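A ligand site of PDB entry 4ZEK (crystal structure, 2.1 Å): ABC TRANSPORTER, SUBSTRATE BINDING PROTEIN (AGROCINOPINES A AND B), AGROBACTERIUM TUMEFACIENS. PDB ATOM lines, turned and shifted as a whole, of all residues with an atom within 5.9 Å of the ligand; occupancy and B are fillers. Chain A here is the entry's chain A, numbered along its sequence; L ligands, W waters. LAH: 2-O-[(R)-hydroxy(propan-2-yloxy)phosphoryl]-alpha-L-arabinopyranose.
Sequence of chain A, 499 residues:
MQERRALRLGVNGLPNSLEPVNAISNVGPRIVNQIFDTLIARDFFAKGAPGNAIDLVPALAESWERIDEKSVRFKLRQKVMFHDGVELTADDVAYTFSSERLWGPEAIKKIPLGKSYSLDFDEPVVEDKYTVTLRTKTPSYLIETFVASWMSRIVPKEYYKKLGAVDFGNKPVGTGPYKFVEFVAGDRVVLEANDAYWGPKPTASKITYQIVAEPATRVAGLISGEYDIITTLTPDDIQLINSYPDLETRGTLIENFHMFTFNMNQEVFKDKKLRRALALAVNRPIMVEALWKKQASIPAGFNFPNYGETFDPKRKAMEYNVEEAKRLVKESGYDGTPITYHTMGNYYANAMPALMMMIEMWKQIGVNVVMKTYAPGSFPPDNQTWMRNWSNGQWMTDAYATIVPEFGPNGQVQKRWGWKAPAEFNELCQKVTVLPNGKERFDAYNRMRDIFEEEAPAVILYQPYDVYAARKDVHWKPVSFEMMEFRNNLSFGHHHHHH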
ATOM      1  N   ILE A  24      -1.091  -9.410 -15.169  1.00  0.00           N
ATOM      2  CA  ILE A  24       0.358  -9.665 -15.018  1.00  0.00           C
ATOM      3  C   ILE A  24       1.186  -8.661 -15.843  1.00  0.00           C
ATOM      4  O   ILE A  24       1.253  -8.739 -17.074  1.00  0.00           O
ATOM      5  CB  ILE A  24       0.776 -11.154 -15.218  1.00  0.00           C
ATOM      6  CG1 ILE A  24       0.227 -12.012 -14.083  1.00  0.00           C
ATOM      7  CG2 ILE A  24       2.319 -11.271 -15.325  1.00  0.00           C
ATOM      8  CD1 ILE A  24       0.258 -13.511 -14.364  1.00  0.00           C
ATOM      9  N   SER A  25       1.797  -7.722 -15.117  1.00  0.00           N
ATOM     10  CA  SER A  25       2.596  -6.627 -15.653  1.00  0.00           C
ATOM     11  C   SER A  25       3.340  -5.996 -14.475  1.00  0.00           C
ATOM     12  O   SER A  25       3.323  -6.558 -13.380  1.00  0.00           O
ATOM     13  CB  SER A  25       1.692  -5.586 -16.308  1.00  0.00           C
ATOM     14  OG  SER A  25       0.738  -5.086 -15.382  1.00  0.00           O
ATOM     15  N   ASN A  26       3.981  -4.835 -14.673  1.00  0.00           N
ATOM     16  CA  ASN A  26       4.663  -4.144 -13.583  1.00  0.00           C
ATOM     17  C   ASN A  26       3.642  -3.347 -12.765  1.00  0.00           C
ATOM     18  O   ASN A  26       3.890  -3.055 -11.608  1.00  0.00           O
ATOM     19  CB  ASN A  26       5.708  -3.160 -14.163  1.00  0.00           C
ATOM     20  CG  ASN A  26       7.022  -3.773 -14.620  1.00  0.00           C
ATOM     21  OD1 ASN A  26       7.243  -4.974 -14.597  1.00  0.00           O
ATOM     22  ND2 ASN A  26       7.923  -2.922 -15.056  1.00  0.00           N
ATOM     23  N   VAL A  27       2.489  -3.038 -13.395  1.00  0.00           N
ATOM     24  CA  VAL A  27       1.427  -2.160 -12.884  1.00  0.00           C
ATOM     25  C   VAL A  27       0.164  -2.810 -12.301  1.00  0.00           C
ATOM     26  O   VAL A  27      -0.539  -2.161 -11.517  1.00  0.00           O
ATOM     27  CB  VAL A  27       1.079  -1.050 -13.929  1.00  0.00           C
ATOM     28  CG1 VAL A  27       2.290  -0.170 -14.213  1.00  0.00           C
ATOM     29  CG2 VAL A  27       0.534  -1.636 -15.217  1.00  0.00           C
ATOM     30  N   TYR A 117       1.813 -19.455 -19.973  1.00  0.00           N
ATOM     31  CA  TYR A 117       2.322 -19.211 -18.620  1.00  0.00           C
ATOM     32  C   TYR A 117       1.957 -20.367 -17.645  1.00  0.00           C
ATOM     33  O   TYR A 117       2.509 -20.429 -16.551  1.00  0.00           O
ATOM     34  CB  TYR A 117       1.793 -17.875 -18.063  1.00  0.00           C
ATOM     35  CG  TYR A 117       2.325 -16.595 -18.662  1.00  0.00           C
ATOM     36  CD1 TYR A 117       3.266 -16.602 -19.682  1.00  0.00           C
ATOM     37  CD2 TYR A 117       1.861 -15.351 -18.231  1.00  0.00           C
ATOM     38  CE1 TYR A 117       3.739 -15.414 -20.250  1.00  0.00           C
ATOM     39  CE2 TYR A 117       2.344 -14.162 -18.770  1.00  0.00           C
ATOM     40  CZ  TYR A 117       3.279 -14.198 -19.790  1.00  0.00           C
ATOM     41  OH  TYR A 117       3.735 -13.016 -20.320  1.00  0.00           O
ATOM     42  N   TRP A 150       1.643 -15.020  -9.038  1.00  0.00           N
ATOM     43  CA  TRP A 150       0.664 -14.110  -9.628  1.00  0.00           C
ATOM     44  C   TRP A 150      -0.269 -14.785 -10.668  1.00  0.00           C
ATOM     45  O   TRP A 150      -1.220 -14.153 -11.125  1.00  0.00           O
ATOM     46  CB  TRP A 150       1.355 -12.862 -10.211  1.00  0.00           C
ATOM     47  CG  TRP A 150       2.466 -13.095 -11.208  1.00  0.00           C
ATOM     48  CD1 TRP A 150       2.850 -14.279 -11.765  1.00  0.00           C
ATOM     49  CD2 TRP A 150       3.314 -12.091 -11.769  1.00  0.00           C
ATOM     50  NE1 TRP A 150       3.867 -14.072 -12.659  1.00  0.00           N
ATOM     51  CE2 TRP A 150       4.212 -12.745 -12.640  1.00  0.00           C
ATOM     52  CE3 TRP A 150       3.411 -10.702 -11.613  1.00  0.00           C
ATOM     53  CZ2 TRP A 150       5.209 -12.051 -13.354  1.00  0.00           C
ATOM     54  CZ3 TRP A 150       4.369 -10.010 -12.351  1.00  0.00           C
ATOM     55  CH2 TRP A 150       5.273 -10.681 -13.184  1.00  0.00           C
ATOM     56  N   ASN A 256      12.956  -9.052 -10.943  1.00  0.00           N
ATOM     57  CA  ASN A 256      12.567  -8.650 -12.289  1.00  0.00           C
ATOM     58  C   ASN A 256      13.809  -8.154 -13.006  1.00  0.00           C
ATOM     59  O   ASN A 256      14.668  -7.532 -12.385  1.00  0.00           O
ATOM     60  CB  ASN A 256      11.542  -7.494 -12.187  1.00  0.00           C
ATOM     61  CG  ASN A 256      11.153  -6.834 -13.494  1.00  0.00           C
ATOM     62  OD1 ASN A 256      11.862  -5.966 -14.040  1.00  0.00           O
ATOM     63  ND2 ASN A 256      10.002  -7.201 -14.022  1.00  0.00           N
ATOM     64  N   MET A 344       7.003   3.022 -24.057  1.00  0.00           N
ATOM     65  CA  MET A 344       5.804   3.672 -23.539  1.00  0.00           C
ATOM     66  C   MET A 344       6.248   4.740 -22.539  1.00  0.00           C
ATOM     67  O   MET A 344       5.965   4.636 -21.341  1.00  0.00           O
ATOM     68  CB  MET A 344       4.900   2.628 -22.869  1.00  0.00           C
ATOM     69  CG  MET A 344       3.448   3.039 -22.741  1.00  0.00           C
ATOM     70  SD  MET A 344       2.606   2.100 -21.448  1.00  0.00           S
ATOM     71  CE  MET A 344       2.689   0.451 -22.132  1.00  0.00           C
ATOM     72  N   TYR A 347       7.376   4.127 -18.577  1.00  0.00           N
ATOM     73  CA  TYR A 347       6.618   3.046 -17.936  1.00  0.00           C
ATOM     74  C   TYR A 347       7.631   2.292 -17.060  1.00  0.00           C
ATOM     75  O   TYR A 347       7.370   2.022 -15.886  1.00  0.00           O
ATOM     76  CB  TYR A 347       5.984   2.125 -19.018  1.00  0.00           C
ATOM     77  CG  TYR A 347       5.272   0.902 -18.479  1.00  0.00           C
ATOM     78  CD1 TYR A 347       3.928   0.956 -18.111  1.00  0.00           C
ATOM     79  CD2 TYR A 347       5.936  -0.318 -18.341  1.00  0.00           C
ATOM     80  CE1 TYR A 347       3.265  -0.177 -17.631  1.00  0.00           C
ATOM     81  CE2 TYR A 347       5.291  -1.444 -17.829  1.00  0.00           C
ATOM     82  CZ  TYR A 347       3.959  -1.376 -17.477  1.00  0.00           C
ATOM     83  OH  TYR A 347       3.301  -2.490 -17.008  1.00  0.00           O
ATOM     84  N   TYR A 348       8.818   2.030 -17.635  1.00  0.00           N
ATOM     85  CA  TYR A 348       9.947   1.444 -16.948  1.00  0.00           C
ATOM     86  C   TYR A 348      10.804   2.587 -16.453  1.00  0.00           C
ATOM     87  O   TYR A 348      10.989   3.566 -17.181  1.00  0.00           O
ATOM     88  CB  TYR A 348      10.789   0.569 -17.900  1.00  0.00           C
ATOM     89  CG  TYR A 348      10.007  -0.578 -18.481  1.00  0.00           C
ATOM     90  CD1 TYR A 348       9.554  -1.626 -17.683  1.00  0.00           C
ATOM     91  CD2 TYR A 348       9.751  -0.647 -19.841  1.00  0.00           C
ATOM     92  CE1 TYR A 348       8.784  -2.659 -18.210  1.00  0.00           C
ATOM     93  CE2 TYR A 348       9.029  -1.712 -20.392  1.00  0.00           C
ATOM     94  CZ  TYR A 348       8.535  -2.698 -19.570  1.00  0.00           C
ATOM     95  OH  TYR A 348       7.814  -3.726 -20.100  1.00  0.00           O
ATOM     96  N   TYR A 374       5.032   5.635 -27.559  1.00  0.00           N
ATOM     97  CA  TYR A 374       3.628   5.254 -27.715  1.00  0.00           C
ATOM     98  C   TYR A 374       2.856   5.451 -26.409  1.00  0.00           C
ATOM     99  O   TYR A 374       3.395   5.204 -25.325  1.00  0.00           O
ATOM    100  CB  TYR A 374       3.441   3.832 -28.310  1.00  0.00           C
ATOM    101  CG  TYR A 374       3.897   2.694 -27.433  1.00  0.00           C
ATOM    102  CD1 TYR A 374       3.003   2.048 -26.576  1.00  0.00           C
ATOM    103  CD2 TYR A 374       5.220   2.249 -27.450  1.00  0.00           C
ATOM    104  CE1 TYR A 374       3.412   0.981 -25.778  1.00  0.00           C
ATOM    105  CE2 TYR A 374       5.645   1.192 -26.644  1.00  0.00           C
ATOM    106  CZ  TYR A 374       4.734   0.566 -25.806  1.00  0.00           C
ATOM    107  OH  TYR A 374       5.129  -0.467 -25.002  1.00  0.00           O
ATOM    108  N   TRP A 390      11.085  -4.085 -22.587  1.00  0.00           N
ATOM    109  CA  TRP A 390      10.235  -5.031 -21.872  1.00  0.00           C
ATOM    110  C   TRP A 390      10.907  -5.357 -20.535  1.00  0.00           C
ATOM    111  O   TRP A 390      11.991  -4.851 -20.239  1.00  0.00           O
ATOM    112  CB  TRP A 390      10.025  -6.313 -22.734  1.00  0.00           C
ATOM    113  CG  TRP A 390       8.918  -7.244 -22.305  1.00  0.00           C
ATOM    114  CD1 TRP A 390       7.793  -6.935 -21.581  1.00  0.00           C
ATOM    115  CD2 TRP A 390       8.813  -8.642 -22.636  1.00  0.00           C
ATOM    116  NE1 TRP A 390       7.019  -8.056 -21.410  1.00  0.00           N
ATOM    117  CE2 TRP A 390       7.609  -9.115 -22.070  1.00  0.00           C
ATOM    118  CE3 TRP A 390       9.619  -9.539 -23.366  1.00  0.00           C
ATOM    119  CZ2 TRP A 390       7.202 -10.451 -22.187  1.00  0.00           C
ATOM    120  CZ3 TRP A 390       9.221 -10.859 -23.469  1.00  0.00           C
ATOM    121  CH2 TRP A 390       8.032 -11.304 -22.892  1.00  0.00           C
ATOM    122  N   SER A 391      10.233  -6.129 -19.703  1.00  0.00           N
ATOM    123  CA  SER A 391      10.716  -6.588 -18.411  1.00  0.00           C
ATOM    124  C   SER A 391      10.114  -7.961 -18.159  1.00  0.00           C
ATOM    125  O   SER A 391       9.072  -8.288 -18.720  1.00  0.00           O
ATOM    126  CB  SER A 391      10.342  -5.610 -17.300  1.00  0.00           C
ATOM    127  OG  SER A 391       9.108  -5.883 -16.663  1.00  0.00           O
ATOM    128  N   ASN A 392      10.806  -8.774 -17.351  1.00  0.00           N
ATOM    129  CA  ASN A 392      10.288 -10.089 -16.984  1.00  0.00           C
ATOM    130  C   ASN A 392      10.428 -10.272 -15.502  1.00  0.00           C
ATOM    131  O   ASN A 392      11.528 -10.188 -14.960  1.00  0.00           O
ATOM    132  CB  ASN A 392      11.006 -11.225 -17.710  1.00  0.00           C
ATOM    133  CG  ASN A 392      10.432 -11.659 -19.042  1.00  0.00           C
ATOM    134  OD1 ASN A 392       9.564 -11.014 -19.624  1.00  0.00           O
ATOM    135  ND2 ASN A 392      10.999 -12.710 -19.594  1.00  0.00           N
ATOM    136  N   GLY A 393       9.293 -10.465 -14.857  1.00  0.00           N
ATOM    137  CA  GLY A 393       9.241 -10.749 -13.433  1.00  0.00           C
ATOM    138  C   GLY A 393       9.525 -12.217 -13.229  1.00  0.00           C
ATOM    139  O   GLY A 393       8.918 -13.041 -13.912  1.00  0.00           O
ATOM    140  N   GLN A 394      10.519 -12.544 -12.399  1.00  0.00           N
ATOM    141  CA  GLN A 394      10.930 -13.934 -12.137  1.00  0.00           C
ATOM    142  C   GLN A 394      10.046 -14.433 -11.013  1.00  0.00           C
ATOM    143  O   GLN A 394      10.332 -14.208  -9.842  1.00  0.00           O
ATOM    144  CB  GLN A 394      12.428 -14.001 -11.798  1.00  0.00           C
ATOM    145  CG  GLN A 394      13.318 -13.331 -12.856  1.00  0.00           C
ATOM    146  CD  GLN A 394      13.043 -13.827 -14.248  1.00  0.00           C
ATOM    147  OE1 GLN A 394      13.283 -14.991 -14.584  1.00  0.00           O
ATOM    148  NE2 GLN A 394      12.482 -12.968 -15.087  1.00  0.00           N
ATOM    149  N   TRP A 395       8.938 -15.066 -11.400  1.00  0.00           N
ATOM    150  CA  TRP A 395       7.836 -15.446 -10.521  1.00  0.00           C
ATOM    151  C   TRP A 395       7.786 -16.833  -9.842  1.00  0.00           C
ATOM    152  O   TRP A 395       6.786 -17.180  -9.225  1.00  0.00           O
ATOM    153  CB  TRP A 395       6.530 -15.125 -11.229  1.00  0.00           C
ATOM    154  CG  TRP A 395       6.376 -15.743 -12.588  1.00  0.00           C
ATOM    155  CD1 TRP A 395       6.781 -15.209 -13.779  1.00  0.00           C
ATOM    156  CD2 TRP A 395       5.634 -16.919 -12.908  1.00  0.00           C
ATOM    157  NE1 TRP A 395       6.378 -16.020 -14.816  1.00  0.00           N
ATOM    158  CE2 TRP A 395       5.659 -17.068 -14.316  1.00  0.00           C
ATOM    159  CE3 TRP A 395       4.992 -17.903 -12.134  1.00  0.00           C
ATOM    160  CZ2 TRP A 395       5.031 -18.136 -14.967  1.00  0.00           C
ATOM    161  CZ3 TRP A 395       4.363 -18.954 -12.783  1.00  0.00           C
ATOM    162  CH2 TRP A 395       4.381 -19.057 -14.186  1.00  0.00           C
ATOM    163  N   THR A 402      11.514 -16.911 -16.025  1.00  0.00           N
ATOM    164  CA  THR A 402      10.631 -16.790 -17.196  1.00  0.00           C
ATOM    165  C   THR A 402      11.196 -17.377 -18.502  1.00  0.00           C
ATOM    166  O   THR A 402      10.557 -17.213 -19.540  1.00  0.00           O
ATOM    167  CB  THR A 402      10.205 -15.325 -17.453  1.00  0.00           C
ATOM    168  OG1 THR A 402      11.372 -14.500 -17.532  1.00  0.00           O
ATOM    169  CG2 THR A 402       9.237 -14.796 -16.412  1.00  0.00           C
ATOM    170  N   GLU A 406       8.185 -17.469 -21.314  1.00  0.00           N
ATOM    171  CA  GLU A 406       8.380 -16.395 -22.287  1.00  0.00           C
ATOM    172  C   GLU A 406       9.146 -16.760 -23.560  1.00  0.00           C
ATOM    173  O   GLU A 406       8.710 -16.390 -24.651  1.00  0.00           O
ATOM    174  CB  GLU A 406       8.956 -15.134 -21.638  1.00  0.00           C
ATOM    175  CG  GLU A 406       8.082 -14.570 -20.521  1.00  0.00           C
ATOM    176  CD  GLU A 406       6.798 -13.861 -20.898  1.00  0.00           C
ATOM    177  OE1 GLU A 406       6.300 -14.014 -22.040  1.00  0.00           O
ATOM    178  OE2 GLU A 406       6.262 -13.155 -20.028  1.00  0.00           O
ATOM    179  N   GLN A 412       5.410 -16.735 -26.282  1.00  0.00           N
ATOM    180  CA  GLN A 412       5.115 -15.616 -27.187  1.00  0.00           C
ATOM    181  C   GLN A 412       6.313 -15.054 -27.959  1.00  0.00           C
ATOM    182  O   GLN A 412       6.112 -14.483 -29.029  1.00  0.00           O
ATOM    183  CB  GLN A 412       4.342 -14.505 -26.449  1.00  0.00           C
ATOM    184  CG  GLN A 412       5.190 -13.719 -25.444  1.00  0.00           C
ATOM    185  CD  GLN A 412       4.437 -12.566 -24.824  1.00  0.00           C
ATOM    186  OE1 GLN A 412       3.831 -11.753 -25.518  1.00  0.00           O
ATOM    187  NE2 GLN A 412       4.501 -12.455 -23.509  1.00  0.00           N
ATOM    188  N   GLU A 482       7.678  -6.993  -8.107  1.00  0.00           N
ATOM    189  CA  GLU A 482       6.919  -5.923  -8.797  1.00  0.00           C
ATOM    190  C   GLU A 482       5.425  -5.821  -8.361  1.00  0.00           C
ATOM    191  O   GLU A 482       4.510  -5.915  -9.190  1.00  0.00           O
ATOM    192  CB  GLU A 482       7.085  -6.015 -10.322  1.00  0.00           C
ATOM    193  CG  GLU A 482       6.400  -7.223 -10.933  1.00  0.00           C
ATOM    194  CD  GLU A 482       6.887  -7.565 -12.312  1.00  0.00           C
ATOM    195  OE1 GLU A 482       6.182  -7.234 -13.291  1.00  0.00           O
ATOM    196  OE2 GLU A 482       7.968  -8.190 -12.412  1.00  0.00           O
HETATM  197  CAA LAH L   1       2.799  -6.301 -20.458  1.00  0.00           C
HETATM  198  CAL LAH L   1       3.733  -5.222 -19.923  1.00  0.00           C
HETATM  199  CAB LAH L   1       3.692  -3.915 -20.653  1.00  0.00           C
HETATM  200  OAJ LAH L   1       5.022  -5.681 -19.654  1.00  0.00           O
HETATM  201  PAQ LAH L   1       5.597  -5.710 -18.197  1.00  0.00           P
HETATM  202  OAG LAH L   1       7.096  -5.558 -18.274  1.00  0.00           O
HETATM  203  OAC LAH L   1       5.016  -4.590 -17.408  1.00  0.00           O
HETATM  204  O2  LAH L   1       5.207  -7.043 -17.445  1.00  0.00           O
HETATM  205  C2  LAH L   1       5.920  -8.302 -17.548  1.00  0.00           C
HETATM  206  C3  LAH L   1       5.107  -9.308 -18.183  1.00  0.00           C
HETATM  207  O3  LAH L   1       4.845  -8.959 -19.599  1.00  0.00           O
HETATM  208  C4  LAH L   1       5.579 -10.639 -18.112  1.00  0.00           C
HETATM  209  O4  LAH L   1       6.697 -10.837 -18.992  1.00  0.00           O
HETATM  210  C5  LAH L   1       6.037 -11.036 -16.728  1.00  0.00           C
HETATM  211  O5  LAH L   1       6.839 -10.033 -16.121  1.00  0.00           O
HETATM  212  C1  LAH L   1       6.275  -8.744 -16.137  1.00  0.00           C
HETATM  213  O1  LAH L   1       7.154  -7.871 -15.556  1.00  0.00           O
HETATM  214  O   HOH W   1       6.319  -3.010 -22.721  1.00  0.00           O
HETATM  215  O   HOH W   2       0.746  -2.903 -19.132  1.00  0.00           O
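OE1 of Glu 482 sits at hydrogen-bond distance from O1 of the ligand (2.5 Å). O4 of the ligand lies within hydrogen-bond range of OE2 of Glu 406. OAG of the ligand lies close to N of Ser 391 (3.5 Å). O of Ser 391 sits close to O4 of the ligand. An oxygen (OAG) of the ligand lies within hydrogen-bond range of the side-chain hydroxyl (OG) of Ser 391 (2.6 Å). OH of Tyr 348 is in hydrogen-bond range of OAG of the ligand (2.7 Å). The side-chain hydroxyl (OH) of Tyr 347 is in hydrogen-bond range of an oxygen (OAC) of the ligand (2.7 Å). N of Gly 393 lies within hydrogen-bond range of O5 of the ligand, at 2.8 Å. The backbone NH (N) of Asn 26 lies within hydrogen-bond range of an oxygen (OAC) of the ligand (2.9 Å). O1 of the ligand is in hydrogen-bond range of OD1 of Asn 26 (3.1 Å). OD1 of Asn 392 lies within hydrogen-bond range of O4 of the ligand (2.9 Å). O3 of the ligand is in hydrogen-bond range of NE1 of Trp 390, at 3.0 Å. The side-chain amide nitrogen of Asn 256 is in hydrogen-bond range of an oxygen (O1) of the ligand, at 3.3 Å.
The side-chain carboxylate (OE2) of Glu 482 sits at hydrogen-bond distance from the side-chain amide nitrogen (ND2) of Asn 256, at 2.8 Å. OE2 of Glu 406 sits at hydrogen-bond distance from OH of Tyr 117 (2.5 Å). OH of Tyr 348 is in hydrogen-bond range of N of Ser 391 (3.4 Å). The side-chain amide oxygen (OD1) of Asn 26 is in hydrogen-bond range of the side-chain hydroxyl (OG) of Ser 391 (2.9 Å). The side-chain amide nitrogen (ND2) of Asn 256 is in hydrogen-bond range of the side-chain hydroxyl (OG) of Ser 391, at 3.1 Å. The backbone NH of Gly 393 sits close to the side-chain amide nitrogen of Asn 256 (3.4 Å). The backbone NH (N) of Val 27 sits close to the side-chain hydroxyl (OG) of Ser 25. The side-chain amide nitrogen (NE2) of Gln 412 sits at hydrogen-bond distance from the side-chain hydroxyl (OH) of Tyr 117 (3.3 Å).
Ile 24 touches the ligand (CG2 to C5, 3.98 Å). Ser 25 touches the ligand. Tyr 117 touches the ligand (OH to C4, 3.7 Å). CH2 of Trp 150 touches O5 of the ligand (3.4 Å). 14 residues have an atom within 4 Å of the ligand: Ile 24, Ser 25, Asn 26, Tyr 117, Trp 150, Asn 256, Tyr 347, Tyr 348, Trp 390, Ser 391, Asn 392, Gly 393, Glu 406 and Glu 482. The nearest printed residue that does not touch the ligand is Met 344 (4.7 Å).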
